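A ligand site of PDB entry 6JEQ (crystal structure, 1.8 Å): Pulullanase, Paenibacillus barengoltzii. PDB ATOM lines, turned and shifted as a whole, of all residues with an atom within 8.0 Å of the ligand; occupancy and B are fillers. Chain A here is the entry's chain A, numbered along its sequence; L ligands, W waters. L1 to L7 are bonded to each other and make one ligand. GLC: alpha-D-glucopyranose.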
ATOM      1  N   GLU A  48      14.778 -13.038   1.545  1.00  0.00           N
ATOM      2  CA  GLU A  48      16.022 -12.642   2.193  1.00  0.00           C
ATOM      3  C   GLU A  48      16.895 -11.727   1.341  1.00  0.00           C
ATOM      4  O   GLU A  48      17.774 -11.068   1.898  1.00  0.00           O
ATOM      5  CB  GLU A  48      16.833 -13.877   2.587  1.00  0.00           C
ATOM      6  CG  GLU A  48      16.231 -14.625   3.776  1.00  0.00           C
ATOM      7  CD  GLU A  48      16.342 -16.140   3.661  1.00  0.00           C
ATOM      8  OE1 GLU A  48      17.489 -16.636   3.630  1.00  0.00           O
ATOM      9  OE2 GLU A  48      15.288 -16.825   3.617  1.00  0.00           O
ATOM     10  N   GLU A  49      16.681 -11.679   0.030  1.00  0.00           N
ATOM     11  CA  GLU A  49      17.541 -10.864  -0.823  1.00  0.00           C
ATOM     12  C   GLU A  49      16.862 -10.609  -2.160  1.00  0.00           C
ATOM     13  O   GLU A  49      16.066 -11.425  -2.639  1.00  0.00           O
ATOM     14  CB  GLU A  49      18.898 -11.545  -1.052  1.00  0.00           C
ATOM     15  CG  GLU A  49      18.767 -12.882  -1.785  1.00  0.00           C
ATOM     16  CD  GLU A  49      20.107 -13.533  -2.082  1.00  0.00           C
ATOM     17  OE1 GLU A  49      21.023 -13.466  -1.217  1.00  0.00           O
ATOM     18  OE2 GLU A  49      20.252 -14.108  -3.171  1.00  0.00           O
ATOM     19  N   THR A  50      17.182  -9.465  -2.773  1.00  0.00           N
ATOM     20  CA  THR A  50      16.760  -9.157  -4.139  1.00  0.00           C
ATOM     21  C   THR A  50      18.002  -8.953  -4.990  1.00  0.00           C
ATOM     22  O   THR A  50      18.934  -8.248  -4.586  1.00  0.00           O
ATOM     23  CB  THR A  50      15.863  -7.922  -4.188  1.00  0.00           C
ATOM     24  OG1 THR A  50      14.688  -8.144  -3.403  1.00  0.00           O
ATOM     25  CG2 THR A  50      15.435  -7.627  -5.639  1.00  0.00           C
ATOM     26  N   ARG A  51      18.017  -9.572  -6.172  1.00  0.00           N
ATOM     27  CA  ARG A  51      19.161  -9.544  -7.068  1.00  0.00           C
ATOM     28  C   ARG A  51      18.819  -8.685  -8.287  1.00  0.00           C
ATOM     29  O   ARG A  51      17.811  -8.931  -8.948  1.00  0.00           O
ATOM     30  CB  ARG A  51      19.554 -10.952  -7.499  1.00  0.00           C
ATOM     31  CG  ARG A  51      19.679 -11.932  -6.325  1.00  0.00           C
ATOM     32  CD  ARG A  51      20.227 -13.289  -6.776  1.00  0.00           C
ATOM     33  NE  ARG A  51      19.321 -13.974  -7.690  1.00  0.00           N
ATOM     34  CZ  ARG A  51      18.233 -14.638  -7.320  1.00  0.00           C
ATOM     35  NH1 ARG A  51      17.898 -14.705  -6.027  1.00  0.00           N
ATOM     36  NH2 ARG A  51      17.469 -15.237  -8.225  1.00  0.00           N
ATOM     37  N   LEU A  78      22.783   2.361  -3.519  1.00  0.00           N
ATOM     38  CA  LEU A  78      23.815   1.336  -3.412  1.00  0.00           C
ATOM     39  C   LEU A  78      24.556   1.166  -4.728  1.00  0.00           C
ATOM     40  O   LEU A  78      23.927   0.959  -5.765  1.00  0.00           O
ATOM     41  CB  LEU A  78      23.183  -0.006  -2.999  1.00  0.00           C
ATOM     42  CG  LEU A  78      22.398   0.093  -1.690  1.00  0.00           C
ATOM     43  CD1 LEU A  78      21.373  -1.004  -1.561  1.00  0.00           C
ATOM     44  CD2 LEU A  78      23.363   0.048  -0.508  1.00  0.00           C
ATOM     45  N   PRO A  79      25.885   1.229  -4.736  1.00  0.00           N
ATOM     46  CA  PRO A  79      26.607   1.062  -6.004  1.00  0.00           C
ATOM     47  C   PRO A  79      26.569  -0.388  -6.465  1.00  0.00           C
ATOM     48  O   PRO A  79      26.656  -1.322  -5.663  1.00  0.00           O
ATOM     49  CB  PRO A  79      28.041   1.497  -5.672  1.00  0.00           C
ATOM     50  CG  PRO A  79      28.175   1.173  -4.201  1.00  0.00           C
ATOM     51  CD  PRO A  79      26.803   1.415  -3.595  1.00  0.00           C
ATOM     52  N   MET A  80      26.423  -0.559  -7.781  1.00  0.00           N
ATOM     53  CA  MET A  80      26.468  -1.877  -8.383  1.00  0.00           C
ATOM     54  C   MET A  80      27.878  -2.235  -8.798  1.00  0.00           C
ATOM     55  O   MET A  80      28.769  -1.366  -8.926  1.00  0.00           O
ATOM     56  CB  MET A  80      25.523  -1.956  -9.594  1.00  0.00           C
ATOM     57  CG  MET A  80      24.087  -1.510  -9.273  1.00  0.00           C
ATOM     58  SD  MET A  80      23.024  -1.504 -10.728  1.00  0.00           S
ATOM     59  CE  MET A  80      22.591  -3.263 -10.847  1.00  0.00           C
ATOM     60  N   LYS A  81      28.090  -3.518  -9.016  1.00  0.00           N
ATOM     61  CA  LYS A  81      29.374  -4.064  -9.422  1.00  0.00           C
ATOM     62  C   LYS A  81      29.366  -4.318 -10.928  1.00  0.00           C
ATOM     63  O   LYS A  81      28.416  -4.902 -11.453  1.00  0.00           O
ATOM     64  CB  LYS A  81      29.665  -5.356  -8.667  1.00  0.00           C
ATOM     65  CG  LYS A  81      30.892  -6.107  -9.131  1.00  0.00           C
ATOM     66  CD  LYS A  81      30.927  -7.483  -8.466  1.00  0.00           C
ATOM     67  CE  LYS A  81      31.751  -8.468  -9.268  1.00  0.00           C
ATOM     68  NZ  LYS A  81      33.160  -8.012  -9.430  1.00  0.00           N
ATOM     69  N   ARG A  82      30.425  -3.890 -11.621  1.00  0.00           N
ATOM     70  CA  ARG A  82      30.531  -4.169 -13.047  1.00  0.00           C
ATOM     71  C   ARG A  82      30.702  -5.675 -13.243  1.00  0.00           C
ATOM     72  O   ARG A  82      31.589  -6.289 -12.641  1.00  0.00           O
ATOM     73  CB  ARG A  82      31.717  -3.410 -13.646  1.00  0.00           C
ATOM     74  CG  ARG A  82      31.825  -3.491 -15.154  1.00  0.00           C
ATOM     75  CD  ARG A  82      30.615  -2.894 -15.812  1.00  0.00           C
ATOM     76  NE  ARG A  82      30.858  -2.581 -17.219  1.00  0.00           N
ATOM     77  CZ  ARG A  82      30.792  -3.468 -18.206  1.00  0.00           C
ATOM     78  NH1 ARG A  82      30.507  -4.749 -17.929  1.00  0.00           N
ATOM     79  NH2 ARG A  82      31.018  -3.099 -19.456  1.00  0.00           N
ATOM     80  N   THR A  89      25.678  -5.750 -11.534  1.00  0.00           N
ATOM     81  CA  THR A  89      24.907  -6.596 -10.617  1.00  0.00           C
ATOM     82  C   THR A  89      24.948  -6.038  -9.204  1.00  0.00           C
ATOM     83  O   THR A  89      25.847  -5.286  -8.818  1.00  0.00           O
ATOM     84  CB  THR A  89      25.417  -8.045 -10.592  1.00  0.00           C
ATOM     85  OG1 THR A  89      26.829  -8.078 -10.332  1.00  0.00           O
ATOM     86  CG2 THR A  89      25.142  -8.696 -11.905  1.00  0.00           C
ATOM     87  N   LEU A  90      23.950  -6.445  -8.414  1.00  0.00           N
ATOM     88  CA  LEU A  90      23.882  -6.082  -7.008  1.00  0.00           C
ATOM     89  C   LEU A  90      22.918  -7.042  -6.331  1.00  0.00           C
ATOM     90  O   LEU A  90      21.827  -7.268  -6.842  1.00  0.00           O
ATOM     91  CB  LEU A  90      23.400  -4.638  -6.794  1.00  0.00           C
ATOM     92  CG  LEU A  90      23.307  -4.224  -5.318  1.00  0.00           C
ATOM     93  CD1 LEU A  90      24.714  -4.139  -4.727  1.00  0.00           C
ATOM     94  CD2 LEU A  90      22.566  -2.914  -5.115  1.00  0.00           C
ATOM     95  N   THR A  91      23.323  -7.577  -5.187  1.00  0.00           N
ATOM     96  CA  THR A  91      22.387  -8.277  -4.316  1.00  0.00           C
ATOM     97  C   THR A  91      22.150  -7.431  -3.069  1.00  0.00           C
ATOM     98  O   THR A  91      23.105  -7.096  -2.354  1.00  0.00           O
ATOM     99  CB  THR A  91      22.918  -9.670  -3.935  1.00  0.00           C
ATOM    100  OG1 THR A  91      23.113 -10.452  -5.121  1.00  0.00           O
ATOM    101  CG2 THR A  91      21.902 -10.376  -3.019  1.00  0.00           C
ATOM    102  N   VAL A  92      20.893  -7.062  -2.819  1.00  0.00           N
ATOM    103  CA  VAL A  92      20.520  -6.319  -1.613  1.00  0.00           C
ATOM    104  C   VAL A  92      20.040  -7.335  -0.587  1.00  0.00           C
ATOM    105  O   VAL A  92      18.999  -7.977  -0.761  1.00  0.00           O
ATOM    106  CB  VAL A  92      19.448  -5.259  -1.907  1.00  0.00           C
ATOM    107  CG1 VAL A  92      19.008  -4.598  -0.618  1.00  0.00           C
ATOM    108  CG2 VAL A  92      20.007  -4.217  -2.849  1.00  0.00           C
ATOM    109  N   ALA A  93      20.805  -7.473   0.492  1.00  0.00           N
ATOM    110  CA  ALA A  93      20.589  -8.537   1.478  1.00  0.00           C
ATOM    111  C   ALA A  93      19.602  -8.059   2.554  1.00  0.00           C
ATOM    112  O   ALA A  93      19.939  -7.864   3.718  1.00  0.00           O
ATOM    113  CB  ALA A  93      21.908  -8.974   2.094  1.00  0.00           C
ATOM    114  N   GLU A  94      18.373  -7.851   2.122  1.00  0.00           N
ATOM    115  CA  GLU A  94      17.284  -7.549   3.033  1.00  0.00           C
ATOM    116  C   GLU A  94      15.979  -7.890   2.316  1.00  0.00           C
ATOM    117  O   GLU A  94      15.979  -8.187   1.118  1.00  0.00           O
ATOM    118  CB  GLU A  94      17.303  -6.082   3.506  1.00  0.00           C
ATOM    119  CG  GLU A  94      16.945  -5.051   2.451  1.00  0.00           C
ATOM    120  CD  GLU A  94      17.115  -3.605   2.945  1.00  0.00           C
ATOM    121  OE1 GLU A  94      18.195  -3.006   2.742  1.00  0.00           O
ATOM    122  OE2 GLU A  94      16.156  -3.062   3.549  1.00  0.00           O
HETATM  123  C1  GLC L   1      33.461  -4.993  -3.177  1.00  0.00           C
HETATM  124  C2  GLC L   1      33.528  -5.386  -4.656  1.00  0.00           C
HETATM  125  C3  GLC L   1      33.868  -6.872  -4.795  1.00  0.00           C
HETATM  126  C4  GLC L   1      35.109  -7.280  -4.002  1.00  0.00           C
HETATM  127  C5  GLC L   1      35.017  -6.749  -2.567  1.00  0.00           C
HETATM  128  C6  GLC L   1      36.336  -6.923  -1.821  1.00  0.00           C
HETATM  129  O2  GLC L   1      32.294  -5.082  -5.286  1.00  0.00           O
HETATM  130  O3  GLC L   1      34.078  -7.230  -6.150  1.00  0.00           O
HETATM  131  O4  GLC L   1      35.164  -8.688  -3.994  1.00  0.00           O
HETATM  132  O5  GLC L   1      34.673  -5.361  -2.529  1.00  0.00           O
HETATM  133  O6  GLC L   1      36.185  -6.453  -0.506  1.00  0.00           O
HETATM  134  C1  GLC L   2      36.476  -9.206  -4.301  1.00  0.00           C
HETATM  135  C2  GLC L   2      36.386 -10.146  -5.493  1.00  0.00           C
HETATM  136  C3  GLC L   2      35.504 -11.343  -5.141  1.00  0.00           C
HETATM  137  C4  GLC L   2      35.971 -12.019  -3.861  1.00  0.00           C
HETATM  138  C5  GLC L   2      36.243 -11.017  -2.742  1.00  0.00           C
HETATM  139  C6  GLC L   2      37.009 -11.694  -1.608  1.00  0.00           C
HETATM  140  O2  GLC L   2      35.880  -9.447  -6.608  1.00  0.00           O
HETATM  141  O3  GLC L   2      35.512 -12.269  -6.203  1.00  0.00           O
HETATM  142  O4  GLC L   2      34.977 -12.929  -3.423  1.00  0.00           O
HETATM  143  O5  GLC L   2      37.017  -9.924  -3.200  1.00  0.00           O
HETATM  144  O6  GLC L   2      36.889 -10.952  -0.413  1.00  0.00           O
HETATM  145  C1  GLC L   3      29.016  -4.739  -0.396  1.00  0.00           C
HETATM  146  C2  GLC L   3      29.055  -4.086  -1.780  1.00  0.00           C
HETATM  147  C3  GLC L   3      30.151  -4.725  -2.623  1.00  0.00           C
HETATM  148  C4  GLC L   3      31.492  -4.776  -1.892  1.00  0.00           C
HETATM  149  C5  GLC L   3      31.364  -5.216  -0.445  1.00  0.00           C
HETATM  150  C6  GLC L   3      32.654  -4.808   0.289  1.00  0.00           C
HETATM  151  O2  GLC L   3      27.797  -4.191  -2.433  1.00  0.00           O
HETATM  152  O3  GLC L   3      30.349  -3.969  -3.787  1.00  0.00           O
HETATM  153  O4  GLC L   3      32.320  -5.672  -2.582  1.00  0.00           O
HETATM  154  O5  GLC L   3      30.275  -4.583   0.225  1.00  0.00           O
HETATM  155  O6  GLC L   3      32.463  -4.965   1.665  1.00  0.00           O
HETATM  156  C1  GLC L   4      35.529 -14.265  -3.308  1.00  0.00           C
HETATM  157  C2  GLC L   4      34.729 -15.202  -4.205  1.00  0.00           C
HETATM  158  C3  GLC L   4      33.272 -15.152  -3.777  1.00  0.00           C
HETATM  159  C4  GLC L   4      33.130 -15.526  -2.312  1.00  0.00           C
HETATM  160  C5  GLC L   4      34.125 -14.769  -1.423  1.00  0.00           C
HETATM  161  C6  GLC L   4      34.230 -15.407  -0.044  1.00  0.00           C
HETATM  162  O2  GLC L   4      34.851 -14.808  -5.552  1.00  0.00           O
HETATM  163  O3  GLC L   4      32.471 -15.987  -4.588  1.00  0.00           O
HETATM  164  O4  GLC L   4      31.810 -15.212  -1.928  1.00  0.00           O
HETATM  165  O5  GLC L   4      35.431 -14.742  -1.974  1.00  0.00           O
HETATM  166  O6  GLC L   4      34.498 -14.413   0.919  1.00  0.00           O
HETATM  167  C1  GLC L   5      25.960  -8.806   1.099  1.00  0.00           C
HETATM  168  C2  GLC L   5      25.407  -7.883   0.013  1.00  0.00           C
HETATM  169  C3  GLC L   5      26.569  -7.232  -0.735  1.00  0.00           C
HETATM  170  C4  GLC L   5      27.546  -6.534   0.223  1.00  0.00           C
HETATM  171  C5  GLC L   5      27.936  -7.479   1.372  1.00  0.00           C
HETATM  172  C6  GLC L   5      28.686  -6.703   2.454  1.00  0.00           C
HETATM  173  O2  GLC L   5      24.607  -8.636  -0.887  1.00  0.00           O
HETATM  174  O3  GLC L   5      26.096  -6.273  -1.664  1.00  0.00           O
HETATM  175  O4  GLC L   5      28.695  -6.140  -0.511  1.00  0.00           O
HETATM  176  O5  GLC L   5      26.777  -8.047   1.986  1.00  0.00           O
HETATM  177  O6  GLC L   5      28.493  -7.321   3.699  1.00  0.00           O
HETATM  178  C1  GLC L   6      31.146 -16.369  -1.360  1.00  0.00           C
HETATM  179  C2  GLC L   6      29.838 -16.567  -2.095  1.00  0.00           C
HETATM  180  C3  GLC L   6      28.886 -15.406  -1.830  1.00  0.00           C
HETATM  181  C4  GLC L   6      28.741 -15.108  -0.344  1.00  0.00           C
HETATM  182  C5  GLC L   6      30.130 -14.989   0.284  1.00  0.00           C
HETATM  183  C6  GLC L   6      30.138 -14.734   1.790  1.00  0.00           C
HETATM  184  O2  GLC L   6      30.090 -16.603  -3.490  1.00  0.00           O
HETATM  185  O3  GLC L   6      27.639 -15.664  -2.425  1.00  0.00           O
HETATM  186  O4  GLC L   6      28.011 -13.885  -0.234  1.00  0.00           O
HETATM  187  O5  GLC L   6      30.884 -16.168   0.026  1.00  0.00           O
HETATM  188  O6  GLC L   6      29.395 -15.755   2.422  1.00  0.00           O
HETATM  189  C1  GLC L   7      26.837 -13.978   0.606  1.00  0.00           C
HETATM  190  C2  GLC L   7      25.623 -13.376  -0.113  1.00  0.00           C
HETATM  191  C3  GLC L   7      25.821 -11.881  -0.373  1.00  0.00           C
HETATM  192  C4  GLC L   7      26.262 -11.137   0.882  1.00  0.00           C
HETATM  193  C5  GLC L   7      27.324 -11.889   1.676  1.00  0.00           C
HETATM  194  C6  GLC L   7      27.434 -11.349   3.107  1.00  0.00           C
HETATM  195  O2  GLC L   7      25.375 -14.058  -1.330  1.00  0.00           O
HETATM  196  O3  GLC L   7      24.615 -11.281  -0.806  1.00  0.00           O
HETATM  197  O4  GLC L   7      26.722  -9.860   0.465  1.00  0.00           O
HETATM  198  O5  GLC L   7      27.018 -13.274   1.818  1.00  0.00           O
HETATM  199  O6  GLC L   7      28.545 -11.966   3.704  1.00  0.00           O
HETATM  200  O   HOH W   1      24.413  -6.351   3.271  1.00  0.00           O
HETATM  201  O   HOH W   2      30.866  -1.109  -2.998  1.00  0.00           O
HETATM  202  O   HOH W   3      28.311  -3.540  -5.743  1.00  0.00           O
HETATM  203  O   HOH W   4      30.234  -7.020  -5.173  1.00  0.00           O
HETATM  204  O   HOH W   5      22.910 -15.244  -1.121  1.00  0.00           O
HETATM  205  O   HOH W   6      22.272 -11.869   0.374  1.00  0.00           O
HETATM  206  O   HOH W   7      23.985  -4.331  -0.776  1.00  0.00           O
HETATM  207  O   HOH W   8      26.065  -7.706  -4.217  1.00  0.00           O
HETATM  208  O   HOH W   9      25.127 -12.444  -3.870  1.00  0.00           O
HETATM  209  O   HOH W  10      26.636  -1.733  -2.885  1.00  0.00           O
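Merely in contact with the ligand: Leu 90. Within 4 Å of the ligand: Lys 81, Leu 90 and Thr 91.
Water W5 lies within hydrogen-bond range of the side-chain carboxylate of Glu 49 (2.6 Å) and an oxygen (O2) of GLC L7 (2.7 Å). Water W10 lies within hydrogen-bond range of an oxygen (O2) of GLC L3 (2.8 Å) and the backbone carbonyl oxygen (O) of Pro 79 (2.8 Å). Water W3 lies within hydrogen-bond range of O of Pro 79, O3 of GLC L3 and N of Lys 81. Water W8 bridges N of Thr 91 (2.9 Å) and O3 of GLC L5 (2.9 Å). Water W7 lies within hydrogen-bond range of an oxygen (O3) of GLC L5 and the backbone carbonyl oxygen (O) of Thr 91. Water W9 lies within hydrogen-bond range of O2 of GLC L7 (3.0 Å) and OG1 of Thr 91 (3.1 Å).
O2 of GLC L5 is in hydrogen-bond range of O of Thr 91 (2.6 Å). An oxygen (O3) of GLC L1 is in hydrogen-bond range of the side-chain amino group (NZ) of Lys 81 (3.5 Å).
N of Lys 81 is in hydrogen-bond range of O of Thr 89, 2.9 Å away.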
